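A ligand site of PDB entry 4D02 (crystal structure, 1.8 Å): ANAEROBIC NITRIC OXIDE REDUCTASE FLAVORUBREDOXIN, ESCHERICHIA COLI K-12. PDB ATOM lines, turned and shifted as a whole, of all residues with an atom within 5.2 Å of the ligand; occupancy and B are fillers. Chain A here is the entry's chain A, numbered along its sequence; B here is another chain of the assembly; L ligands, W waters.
OG of Ser 313 lies within hydrogen-bond range of O8 of the ligand, 2.8 Å away.
The backbone NH (N) of Trp 348 sits at hydrogen-bond distance from an oxygen (O1) of the ligand (2.7 Å).
N of Thr 265 is in hydrogen-bond range of O7 of the ligand (2.7 Å).
OG1 of Thr 260 sits at hydrogen-bond distance from O7 of the ligand, 2.7 Å away.
N1 of the ligand lies within hydrogen-bond range of N of Gly 347.
The backbone NH (N) of Asn 317 lies within hydrogen-bond range of an oxygen (O2) of the ligand, at 2.8 Å.
N of Ser 349 sits at hydrogen-bond distance from O1 of the ligand, at 3.2 Å.
The side-chain hydroxyl of Ser 262 lies within hydrogen-bond range of an oxygen (O9) of the ligand (2.6 Å).
An oxygen (O5) of the ligand lies within hydrogen-bond range of the side-chain hydroxyl of Ser 345 (2.7 Å).
N of Asn 264 lies within hydrogen-bond range of O9 of the ligand (2.9 Å).
The backbone NH of Asn 316 is in hydrogen-bond range of a nitrogen (N3) of the ligand (3.0 Å).
The side-chain amide nitrogen of Asn 264 lies within hydrogen-bond range of an oxygen (O5) of the ligand, at 2.8 Å.
N of Ser 262 lies within hydrogen-bond range of O9 of the ligand.
N of Asn 263 lies within hydrogen-bond range of O9 of the ligand (3.0 Å).
O8 of the ligand sits at hydrogen-bond distance from N of Met 261, at 2.6 Å.
An oxygen (O1) of the ligand lies within hydrogen-bond range of the backbone NH of Gly 350, at 2.8 Å.
An oxygen (O3) of the ligand lies within hydrogen-bond range of the backbone carbonyl oxygen (O) of Thr 314 (3.0 Å).
O7 of the ligand sits at hydrogen-bond distance from OG1 of Thr 265, 2.6 Å away.
O of Trp 375 sits at hydrogen-bond distance from OG of Ser 345 (2.7 Å).
The side-chain hydroxyl (OG1) of Thr 265 is in hydrogen-bond range of the backbone NH (N) of Ser 345, 3.3 Å away.
The backbone NH (N) of Asn 264 lies within hydrogen-bond range of the side-chain hydroxyl (OG1) of Thr 260, 3.5 Å away.
N of Asn 263 sits at hydrogen-bond distance from OG1 of Thr 260 (2.9 Å).
N of Trp 375 is in hydrogen-bond range of O of His 346, at 2.8 Å.
OD1 of Asn 264 is in hydrogen-bond range of NE of Arg 376, 2.9 Å away.
The indole nitrogen (NE1) of Trp 375 lies close to the backbone carbonyl oxygen (O) of Gly 347, at 3.4 Å.
The side-chain amide oxygen of Asn 263 lies within hydrogen-bond range of the guanidinium group of Arg 266, 3.3 Å away.
Residues that only touch the ligand: Met 315, His 346, Trp 375, His 23 of chain B, Glu 81 of chain B and Trp 148 of chain B.
Of the 28 residues printed, 21 come within 4 Å of the ligand.
Water W1 bridges an oxygen (O4) of the ligand and the side-chain hydroxyl (OG) of Ser 262.
Water W2 lies within hydrogen-bond range of an oxygen (O4) of the ligand (2.7 Å), the side-chain hydroxyl (OG) of Ser 262 (2.8 Å), a ring nitrogen (NE2) of His 113 of chain B (2.8 Å) and the side-chain amide nitrogen (ND2) of Asn 264 (2.9 Å).
Water W3 lies within hydrogen-bond range of OG of Ser 349 (2.6 Å), OD1 of Asn 317 (2.8 Å), N2 of the ligand (2.8 Å) and O of Gly 350 (2.8 Å).
Water W5 lies within hydrogen-bond range of N3 of the ligand (3.1 Å) and OD1 of Asn 316 (3.4 Å).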
ATOM      1  N   ASP A 259      20.189 -10.665  37.938  1.00  0.00           N
ATOM      2  CA  ASP A 259      21.139  -9.610  37.622  1.00  0.00           C
ATOM      3  C   ASP A 259      20.820  -9.196  36.191  1.00  0.00           C
ATOM      4  O   ASP A 259      20.104  -9.911  35.482  1.00  0.00           O
ATOM      5  CB  ASP A 259      22.593 -10.076  37.782  1.00  0.00           C
ATOM      6  CG  ASP A 259      23.557  -8.924  38.078  1.00  0.00           C
ATOM      7  OD1 ASP A 259      23.244  -7.759  37.757  1.00  0.00           O
ATOM      8  OD2 ASP A 259      24.642  -9.194  38.642  1.00  0.00           O
ATOM      9  N   THR A 260      21.332  -8.047  35.777  1.00  0.00           N
ATOM     10  CA  THR A 260      20.953  -7.470  34.498  1.00  0.00           C
ATOM     11  C   THR A 260      22.033  -6.490  34.035  1.00  0.00           C
ATOM     12  O   THR A 260      22.665  -5.822  34.856  1.00  0.00           O
ATOM     13  CB  THR A 260      19.565  -6.762  34.609  1.00  0.00           C
ATOM     14  OG1 THR A 260      19.159  -6.262  33.336  1.00  0.00           O
ATOM     15  CG2 THR A 260      19.603  -5.621  35.636  1.00  0.00           C
ATOM     16  N   MET A 261      22.269  -6.428  32.733  1.00  0.00           N
ATOM     17  CA  MET A 261      23.294  -5.525  32.203  1.00  0.00           C
ATOM     18  C   MET A 261      22.672  -4.259  31.615  1.00  0.00           C
ATOM     19  O   MET A 261      23.295  -3.203  31.620  1.00  0.00           O
ATOM     20  CB  MET A 261      24.143  -6.231  31.136  1.00  0.00           C
ATOM     21  CG  MET A 261      24.989  -7.362  31.684  1.00  0.00           C
ATOM     22  SD  MET A 261      25.985  -8.192  30.417  1.00  0.00           S
ATOM     23  CE  MET A 261      24.706  -8.954  29.414  1.00  0.00           C
ATOM     24  N   SER A 262      21.449  -4.367  31.113  1.00  0.00           N
ATOM     25  CA  SER A 262      20.817  -3.214  30.473  1.00  0.00           C
ATOM     26  C   SER A 262      19.334  -3.129  30.815  1.00  0.00           C
ATOM     27  O   SER A 262      18.561  -2.549  30.066  1.00  0.00           O
ATOM     28  CB  SER A 262      21.008  -3.275  28.945  1.00  0.00           C
ATOM     29  OG  SER A 262      20.612  -4.529  28.413  1.00  0.00           O
ATOM     30  N   ASN A 263      18.971  -3.741  31.940  1.00  0.00           N
ATOM     31  CA  ASN A 263      17.663  -3.586  32.582  1.00  0.00           C
ATOM     32  C   ASN A 263      16.546  -4.405  31.946  1.00  0.00           C
ATOM     33  O   ASN A 263      15.403  -4.326  32.373  1.00  0.00           O
ATOM     34  CB  ASN A 263      17.251  -2.111  32.605  1.00  0.00           C
ATOM     35  CG  ASN A 263      16.471  -1.753  33.821  1.00  0.00           C
ATOM     36  OD1 ASN A 263      16.912  -1.994  34.952  1.00  0.00           O
ATOM     37  ND2 ASN A 263      15.289  -1.166  33.630  1.00  0.00           N
ATOM     38  N   ASN A 264      16.872  -5.205  30.932  1.00  0.00           N
ATOM     39  CA  ASN A 264      15.842  -5.985  30.248  1.00  0.00           C
ATOM     40  C   ASN A 264      15.242  -7.082  31.137  1.00  0.00           C
ATOM     41  O   ASN A 264      14.027  -7.245  31.214  1.00  0.00           O
ATOM     42  CB  ASN A 264      16.395  -6.579  28.951  1.00  0.00           C
ATOM     43  CG  ASN A 264      16.801  -5.504  27.957  1.00  0.00           C
ATOM     44  OD1 ASN A 264      16.240  -4.402  27.956  1.00  0.00           O
ATOM     45  ND2 ASN A 264      17.775  -5.812  27.112  1.00  0.00           N
ATOM     46  N   THR A 265      16.113  -7.830  31.815  1.00  0.00           N
ATOM     47  CA  THR A 265      15.676  -8.860  32.748  1.00  0.00           C
ATOM     48  C   THR A 265      14.968  -8.231  33.953  1.00  0.00           C
ATOM     49  O   THR A 265      14.074  -8.837  34.562  1.00  0.00           O
ATOM     50  CB  THR A 265      16.885  -9.717  33.204  1.00  0.00           C
ATOM     51  OG1 THR A 265      17.514 -10.299  32.061  1.00  0.00           O
ATOM     52  CG2 THR A 265      16.470 -10.828  34.160  1.00  0.00           C
ATOM     53  N   ARG A 266      15.340  -6.986  34.276  1.00  0.00           N
ATOM     54  CA  ARG A 266      14.640  -6.255  35.334  1.00  0.00           C
ATOM     55  C   ARG A 266      13.199  -5.986  34.932  1.00  0.00           C
ATOM     56  O   ARG A 266      12.278  -6.167  35.736  1.00  0.00           O
ATOM     57  CB  ARG A 266      15.337  -4.942  35.654  1.00  0.00           C
ATOM     58  CG  ARG A 266      14.658  -4.184  36.778  1.00  0.00           C
ATOM     59  CD  ARG A 266      13.829  -3.002  36.299  1.00  0.00           C
ATOM     60  NE  ARG A 266      13.345  -2.210  37.424  1.00  0.00           N
ATOM     61  CZ  ARG A 266      14.005  -1.199  37.975  1.00  0.00           C
ATOM     62  NH1 ARG A 266      15.183  -0.836  37.492  1.00  0.00           N
ATOM     63  NH2 ARG A 266      13.486  -0.550  39.022  1.00  0.00           N
ATOM     64  N   SER A 313      20.511 -12.496  32.106  1.00  0.00           N
ATOM     65  CA  SER A 313      20.673 -12.427  30.672  1.00  0.00           C
ATOM     66  C   SER A 313      21.824 -13.353  30.274  1.00  0.00           C
ATOM     67  O   SER A 313      22.484 -13.931  31.144  1.00  0.00           O
ATOM     68  CB  SER A 313      20.933 -11.003  30.206  1.00  0.00           C
ATOM     69  OG  SER A 313      21.962 -10.403  30.990  1.00  0.00           O
ATOM     70  N   THR A 314      22.067 -13.489  28.985  1.00  0.00           N
ATOM     71  CA  THR A 314      23.223 -14.241  28.523  1.00  0.00           C
ATOM     72  C   THR A 314      24.393 -13.293  28.333  1.00  0.00           C
ATOM     73  O   THR A 314      24.274 -12.242  27.695  1.00  0.00           O
ATOM     74  CB  THR A 314      22.936 -15.016  27.224  1.00  0.00           C
ATOM     75  OG1 THR A 314      21.873 -15.957  27.443  1.00  0.00           O
ATOM     76  CG2 THR A 314      24.178 -15.770  26.774  1.00  0.00           C
ATOM     77  N   MET A 315      25.537 -13.663  28.907  1.00  0.00           N
ATOM     78  CA  MET A 315      26.751 -12.868  28.865  1.00  0.00           C
ATOM     79  C   MET A 315      27.916 -13.766  28.455  1.00  0.00           C
ATOM     80  O   MET A 315      28.338 -14.618  29.233  1.00  0.00           O
ATOM     81  CB  MET A 315      26.998 -12.226  30.236  1.00  0.00           C
ATOM     82  CG  MET A 315      28.294 -11.435  30.361  1.00  0.00           C
ATOM     83  SD  MET A 315      28.584 -10.970  32.091  1.00  0.00           S
ATOM     84  CE  MET A 315      30.050  -9.945  31.954  1.00  0.00           C
ATOM     85  N   ASN A 316      28.410 -13.577  27.236  1.00  0.00           N
ATOM     86  CA  ASN A 316      29.483 -14.399  26.677  1.00  0.00           C
ATOM     87  C   ASN A 316      29.130 -15.893  26.776  1.00  0.00           C
ATOM     88  O   ASN A 316      29.933 -16.686  27.248  1.00  0.00           O
ATOM     89  CB  ASN A 316      30.815 -14.123  27.391  1.00  0.00           C
ATOM     90  CG  ASN A 316      31.198 -12.643  27.385  1.00  0.00           C
ATOM     91  OD1 ASN A 316      31.029 -11.945  26.376  1.00  0.00           O
ATOM     92  ND2 ASN A 316      31.703 -12.158  28.519  1.00  0.00           N
ATOM     93  N   ASN A 317      27.906 -16.213  26.357  1.00  0.00           N
ATOM     94  CA  ASN A 317      27.395 -17.587  26.328  1.00  0.00           C
ATOM     95  C   ASN A 317      27.259 -18.275  27.674  1.00  0.00           C
ATOM     96  O   ASN A 317      27.035 -19.481  27.739  1.00  0.00           O
ATOM     97  CB  ASN A 317      28.249 -18.460  25.404  1.00  0.00           C
ATOM     98  CG  ASN A 317      28.393 -17.864  24.030  1.00  0.00           C
ATOM     99  OD1 ASN A 317      27.416 -17.758  23.290  1.00  0.00           O
ATOM    100  ND2 ASN A 317      29.602 -17.452  23.674  1.00  0.00           N
ATOM    101  N   MET A 320      25.178 -14.573  34.123  1.00  0.00           N
ATOM    102  CA  MET A 320      25.899 -13.518  34.816  1.00  0.00           C
ATOM    103  C   MET A 320      26.512 -14.092  36.089  1.00  0.00           C
ATOM    104  O   MET A 320      25.901 -14.933  36.762  1.00  0.00           O
ATOM    105  CB  MET A 320      24.965 -12.352  35.096  1.00  0.00           C
ATOM    106  CG  MET A 320      24.583 -11.613  33.808  1.00  0.00           C
ATOM    107  SD  MET A 320      23.629 -10.108  34.091  1.00  0.00           S
ATOM    108  CE  MET A 320      24.894  -9.007  34.757  1.00  0.00           C
ATOM    109  N   SER A 345      16.659 -12.240  29.509  1.00  0.00           N
ATOM    110  CA  SER A 345      16.723 -11.751  28.144  1.00  0.00           C
ATOM    111  C   SER A 345      18.008 -12.208  27.470  1.00  0.00           C
ATOM    112  O   SER A 345      18.963 -12.613  28.137  1.00  0.00           O
ATOM    113  CB  SER A 345      16.617 -10.228  28.125  1.00  0.00           C
ATOM    114  OG  SER A 345      16.689  -9.736  26.796  1.00  0.00           O
ATOM    115  N   HIS A 346      18.029 -12.144  26.148  1.00  0.00           N
ATOM    116  CA  HIS A 346      19.221 -12.462  25.387  1.00  0.00           C
ATOM    117  C   HIS A 346      19.234 -11.626  24.108  1.00  0.00           C
ATOM    118  O   HIS A 346      18.188 -11.109  23.686  1.00  0.00           O
ATOM    119  CB  HIS A 346      19.243 -13.946  25.033  1.00  0.00           C
ATOM    120  CG  HIS A 346      18.145 -14.333  24.098  1.00  0.00           C
ATOM    121  ND1 HIS A 346      16.847 -14.547  24.521  1.00  0.00           N
ATOM    122  CD2 HIS A 346      18.134 -14.499  22.749  1.00  0.00           C
ATOM    123  CE1 HIS A 346      16.096 -14.844  23.479  1.00  0.00           C
ATOM    124  NE2 HIS A 346      16.848 -14.827  22.390  1.00  0.00           N
ATOM    125  N   GLY A 347      20.397 -11.524  23.484  1.00  0.00           N
ATOM    126  CA  GLY A 347      20.543 -10.722  22.289  1.00  0.00           C
ATOM    127  C   GLY A 347      20.487 -11.529  20.995  1.00  0.00           C
ATOM    128  O   GLY A 347      19.900 -11.090  20.005  1.00  0.00           O
ATOM    129  N   TRP A 348      21.120 -12.691  20.988  1.00  0.00           N
ATOM    130  CA  TRP A 348      21.106 -13.506  19.781  1.00  0.00           C
ATOM    131  C   TRP A 348      20.865 -14.992  20.101  1.00  0.00           C
ATOM    132  O   TRP A 348      19.725 -15.437  20.104  1.00  0.00           O
ATOM    133  CB  TRP A 348      22.384 -13.285  18.960  1.00  0.00           C
ATOM    134  CG  TRP A 348      23.689 -13.224  19.705  1.00  0.00           C
ATOM    135  CD1 TRP A 348      24.638 -14.210  19.788  1.00  0.00           C
ATOM    136  CD2 TRP A 348      24.235 -12.104  20.435  1.00  0.00           C
ATOM    137  NE1 TRP A 348      25.715 -13.779  20.526  1.00  0.00           N
ATOM    138  CE2 TRP A 348      25.487 -12.500  20.936  1.00  0.00           C
ATOM    139  CE3 TRP A 348      23.765 -10.818  20.710  1.00  0.00           C
ATOM    140  CZ2 TRP A 348      26.292 -11.645  21.704  1.00  0.00           C
ATOM    141  CZ3 TRP A 348      24.561  -9.981  21.476  1.00  0.00           C
ATOM    142  CH2 TRP A 348      25.805 -10.394  21.961  1.00  0.00           C
ATOM    143  N   SER A 349      21.917 -15.759  20.384  1.00  0.00           N
ATOM    144  CA  SER A 349      21.738 -17.195  20.569  1.00  0.00           C
ATOM    145  C   SER A 349      21.333 -17.570  22.008  1.00  0.00           C
ATOM    146  O   SER A 349      20.875 -18.682  22.243  1.00  0.00           O
ATOM    147  CB  SER A 349      22.991 -17.958  20.147  1.00  0.00           C
ATOM    148  OG  SER A 349      24.156 -17.383  20.710  1.00  0.00           O
ATOM    149  N   GLY A 350      21.481 -16.648  22.954  1.00  0.00           N
ATOM    150  CA  GLY A 350      21.089 -16.897  24.325  1.00  0.00           C
ATOM    151  C   GLY A 350      21.711 -18.131  24.930  1.00  0.00           C
ATOM    152  O   GLY A 350      22.815 -18.525  24.562  1.00  0.00           O
ATOM    153  N   LYS A 374      13.687 -11.546  23.938  1.00  0.00           N
ATOM    154  CA  LYS A 374      14.823 -11.062  23.164  1.00  0.00           C
ATOM    155  C   LYS A 374      14.981  -9.549  23.317  1.00  0.00           C
ATOM    156  O   LYS A 374      14.024  -8.809  23.137  1.00  0.00           O
ATOM    157  CB  LYS A 374      14.660 -11.429  21.690  1.00  0.00           C
ATOM    158  CG  LYS A 374      15.927 -11.259  20.879  1.00  0.00           C
ATOM    159  CD  LYS A 374      15.687 -11.647  19.442  1.00  0.00           C
ATOM    160  CE  LYS A 374      16.959 -11.560  18.638  1.00  0.00           C
ATOM    161  NZ  LYS A 374      16.702 -11.814  17.204  1.00  0.00           N
ATOM    162  N   TRP A 375      16.193  -9.121  23.637  1.00  0.00           N
ATOM    163  CA  TRP A 375      16.480  -7.707  23.869  1.00  0.00           C
ATOM    164  C   TRP A 375      15.491  -7.102  24.870  1.00  0.00           C
ATOM    165  O   TRP A 375      15.151  -7.735  25.867  1.00  0.00           O
ATOM    166  CB  TRP A 375      16.454  -6.916  22.556  1.00  0.00           C
ATOM    167  CG  TRP A 375      17.433  -7.362  21.495  1.00  0.00           C
ATOM    168  CD1 TRP A 375      17.133  -7.841  20.254  1.00  0.00           C
ATOM    169  CD2 TRP A 375      18.872  -7.346  21.577  1.00  0.00           C
ATOM    170  NE1 TRP A 375      18.286  -8.124  19.557  1.00  0.00           N
ATOM    171  CE2 TRP A 375      19.366  -7.837  20.355  1.00  0.00           C
ATOM    172  CE3 TRP A 375      19.780  -6.966  22.564  1.00  0.00           C
ATOM    173  CZ2 TRP A 375      20.729  -7.947  20.082  1.00  0.00           C
ATOM    174  CZ3 TRP A 375      21.150  -7.080  22.298  1.00  0.00           C
ATOM    175  CH2 TRP A 375      21.608  -7.563  21.068  1.00  0.00           C
ATOM    176  N   ARG A 376      15.028  -5.886  24.600  1.00  0.00           N
ATOM    177  CA  ARG A 376      14.127  -5.193  25.522  1.00  0.00           C
ATOM    178  C   ARG A 376      12.659  -5.514  25.244  1.00  0.00           C
ATOM    179  O   ARG A 376      12.176  -5.321  24.135  1.00  0.00           O
ATOM    180  CB  ARG A 376      14.370  -3.679  25.453  1.00  0.00           C
ATOM    181  CG  ARG A 376      13.509  -2.850  26.401  1.00  0.00           C
ATOM    182  CD  ARG A 376      14.156  -1.481  26.652  1.00  0.00           C
ATOM    183  NE  ARG A 376      15.510  -1.684  27.174  1.00  0.00           N
ATOM    184  CZ  ARG A 376      16.496  -0.794  27.060  1.00  0.00           C
ATOM    185  NH1 ARG A 376      16.298   0.365  26.447  1.00  0.00           N
ATOM    186  NH2 ARG A 376      17.695  -1.094  27.559  1.00  0.00           N
ATOM    187  N   HIS B  23      27.515  -2.344  32.200  1.00  0.00           N
ATOM    188  CA  HIS B  23      27.002  -3.709  32.093  1.00  0.00           C
ATOM    189  C   HIS B  23      26.544  -4.218  33.461  1.00  0.00           C
ATOM    190  O   HIS B  23      27.041  -5.226  33.955  1.00  0.00           O
ATOM    191  CB  HIS B  23      28.078  -4.646  31.526  1.00  0.00           C
ATOM    192  CG  HIS B  23      28.491  -4.315  30.127  1.00  0.00           C
ATOM    193  ND1 HIS B  23      29.687  -4.738  29.585  1.00  0.00           N
ATOM    194  CD2 HIS B  23      27.869  -3.609  29.155  1.00  0.00           C
ATOM    195  CE1 HIS B  23      29.788  -4.294  28.347  1.00  0.00           C
ATOM    196  NE2 HIS B  23      28.699  -3.610  28.062  1.00  0.00           N
ATOM    197  N   GLU B  81      24.099  -0.912  20.938  1.00  0.00           N
ATOM    198  CA  GLU B  81      24.072  -0.966  22.396  1.00  0.00           C
ATOM    199  C   GLU B  81      23.647   0.401  22.957  1.00  0.00           C
ATOM    200  O   GLU B  81      23.914   1.440  22.349  1.00  0.00           O
ATOM    201  CB  GLU B  81      25.433  -1.380  22.952  1.00  0.00           C
ATOM    202  CG  GLU B  81      25.389  -1.799  24.409  1.00  0.00           C
ATOM    203  CD  GLU B  81      26.582  -2.643  24.830  1.00  0.00           C
ATOM    204  OE1 GLU B  81      27.537  -2.775  24.026  1.00  0.00           O
ATOM    205  OE2 GLU B  81      26.550  -3.190  25.945  1.00  0.00           O
ATOM    206  N   HIS B 113      15.780  -2.692  20.918  1.00  0.00           N
ATOM    207  CA  HIS B 113      15.856  -1.675  21.959  1.00  0.00           C
ATOM    208  C   HIS B 113      14.830  -0.550  21.805  1.00  0.00           C
ATOM    209  O   HIS B 113      14.336  -0.023  22.795  1.00  0.00           O
ATOM    210  CB  HIS B 113      17.255  -1.055  22.007  1.00  0.00           C
ATOM    211  CG  HIS B 113      18.306  -1.983  22.526  1.00  0.00           C
ATOM    212  ND1 HIS B 113      18.930  -2.920  21.740  1.00  0.00           N
ATOM    213  CD2 HIS B 113      18.846  -2.107  23.765  1.00  0.00           C
ATOM    214  CE1 HIS B 113      19.815  -3.579  22.469  1.00  0.00           C
ATOM    215  NE2 HIS B 113      19.772  -3.111  23.703  1.00  0.00           N
ATOM    216  N   HIS B 147      31.891  -6.005  19.137  1.00  0.00           N
ATOM    217  CA  HIS B 147      31.718  -7.176  19.990  1.00  0.00           C
ATOM    218  C   HIS B 147      30.287  -7.748  19.965  1.00  0.00           C
ATOM    219  O   HIS B 147      29.980  -8.708  20.676  1.00  0.00           O
ATOM    220  CB  HIS B 147      32.096  -6.827  21.432  1.00  0.00           C
ATOM    221  CG  HIS B 147      31.203  -5.799  22.052  1.00  0.00           C
ATOM    222  ND1 HIS B 147      30.333  -6.088  23.078  1.00  0.00           N
ATOM    223  CD2 HIS B 147      31.043  -4.481  21.773  1.00  0.00           C
ATOM    224  CE1 HIS B 147      29.667  -4.990  23.412  1.00  0.00           C
ATOM    225  NE2 HIS B 147      30.085  -4.002  22.639  1.00  0.00           N
ATOM    226  N   TRP B 148      29.418  -7.155  19.147  1.00  0.00           N
ATOM    227  CA  TRP B 148      28.044  -7.641  18.997  1.00  0.00           C
ATOM    228  C   TRP B 148      27.807  -8.099  17.563  1.00  0.00           C
ATOM    229  O   TRP B 148      28.552  -7.725  16.670  1.00  0.00           O
ATOM    230  CB  TRP B 148      27.027  -6.554  19.359  1.00  0.00           C
ATOM    231  CG  TRP B 148      26.627  -6.498  20.788  1.00  0.00           C
ATOM    232  CD1 TRP B 148      27.217  -7.140  21.848  1.00  0.00           C
ATOM    233  CD2 TRP B 148      25.520  -5.770  21.337  1.00  0.00           C
ATOM    234  NE1 TRP B 148      26.554  -6.849  23.016  1.00  0.00           N
ATOM    235  CE2 TRP B 148      25.499  -6.012  22.731  1.00  0.00           C
ATOM    236  CE3 TRP B 148      24.542  -4.933  20.780  1.00  0.00           C
ATOM    237  CZ2 TRP B 148      24.543  -5.441  23.576  1.00  0.00           C
ATOM    238  CZ3 TRP B 148      23.575  -4.368  21.630  1.00  0.00           C
ATOM    239  CH2 TRP B 148      23.593  -4.629  23.011  1.00  0.00           C
HETATM  240  N1  LIG L   1      23.412 -12.220  23.942  1.00  0.00           N
HETATM  241  C1  LIG L   1      23.434 -13.526  23.517  1.00  0.00           C
HETATM  242  O1  LIG L   1      22.445 -14.011  22.958  1.00  0.00           O
HETATM  243  N2  LIG L   1      24.563 -14.302  23.719  1.00  0.00           N
HETATM  244  C2  LIG L   1      25.678 -13.788  24.345  1.00  0.00           C
HETATM  245  O2  LIG L   1      26.664 -14.506  24.500  1.00  0.00           O
HETATM  246  C3  LIG L   1      25.659 -12.462  24.779  1.00  0.00           C
HETATM  247  N3  LIG L   1      26.762 -11.896  25.401  1.00  0.00           N
HETATM  248  C4  LIG L   1      26.721 -10.581  25.833  1.00  0.00           C
HETATM  249  C5  LIG L   1      27.822 -10.017  26.483  1.00  0.00           C
HETATM  250  C6  LIG L   1      27.786  -8.692  26.901  1.00  0.00           C
HETATM  251  C7  LIG L   1      28.965  -8.070  27.589  1.00  0.00           C
HETATM  252  C8  LIG L   1      26.647  -7.920  26.677  1.00  0.00           C
HETATM  253  C9  LIG L   1      26.601  -6.492  27.146  1.00  0.00           C
HETATM  254  C10 LIG L   1      25.545  -8.485  26.041  1.00  0.00           C
HETATM  255  C11 LIG L   1      25.582  -9.809  25.609  1.00  0.00           C
HETATM  256  N4  LIG L   1      24.479 -10.375  24.986  1.00  0.00           N
HETATM  257  C12 LIG L   1      24.513 -11.688  24.576  1.00  0.00           C
HETATM  258  C13 LIG L   1      23.229  -9.587  24.735  1.00  0.00           C
HETATM  259  C14 LIG L   1      22.377  -9.513  25.996  1.00  0.00           C
HETATM  260  O3  LIG L   1      22.016 -10.813  26.443  1.00  0.00           O
HETATM  261  C15 LIG L   1      21.150  -8.671  25.658  1.00  0.00           C
HETATM  262  O4  LIG L   1      21.574  -7.329  25.573  1.00  0.00           O
HETATM  263  C16 LIG L   1      20.058  -8.833  26.709  1.00  0.00           C
HETATM  264  O5  LIG L   1      18.866  -8.277  26.216  1.00  0.00           O
HETATM  265  C17 LIG L   1      20.459  -8.102  27.961  1.00  0.00           C
HETATM  266  O6  LIG L   1      19.537  -8.365  29.000  1.00  0.00           O
HETATM  267  P1  LIG L   1      19.740  -7.565  30.381  1.00  0.00           P
HETATM  268  O7  LIG L   1      18.764  -8.083  31.411  1.00  0.00           O
HETATM  269  O8  LIG L   1      21.167  -7.754  30.838  1.00  0.00           O
HETATM  270  O9  LIG L   1      19.490  -6.097  30.101  1.00  0.00           O
HETATM  271  O   HOH W   1      23.041  -5.951  27.409  1.00  0.00           O
HETATM  272  O   HOH W   2      20.145  -5.002  25.720  1.00  0.00           O
HETATM  273  O   HOH W   3      24.760 -17.034  23.239  1.00  0.00           O
HETATM  274  O   HOH W   4      30.323  -8.282  24.616  1.00  0.00           O
HETATM  275  O   HOH W   5      29.178 -12.756  23.580  1.00  0.00           O
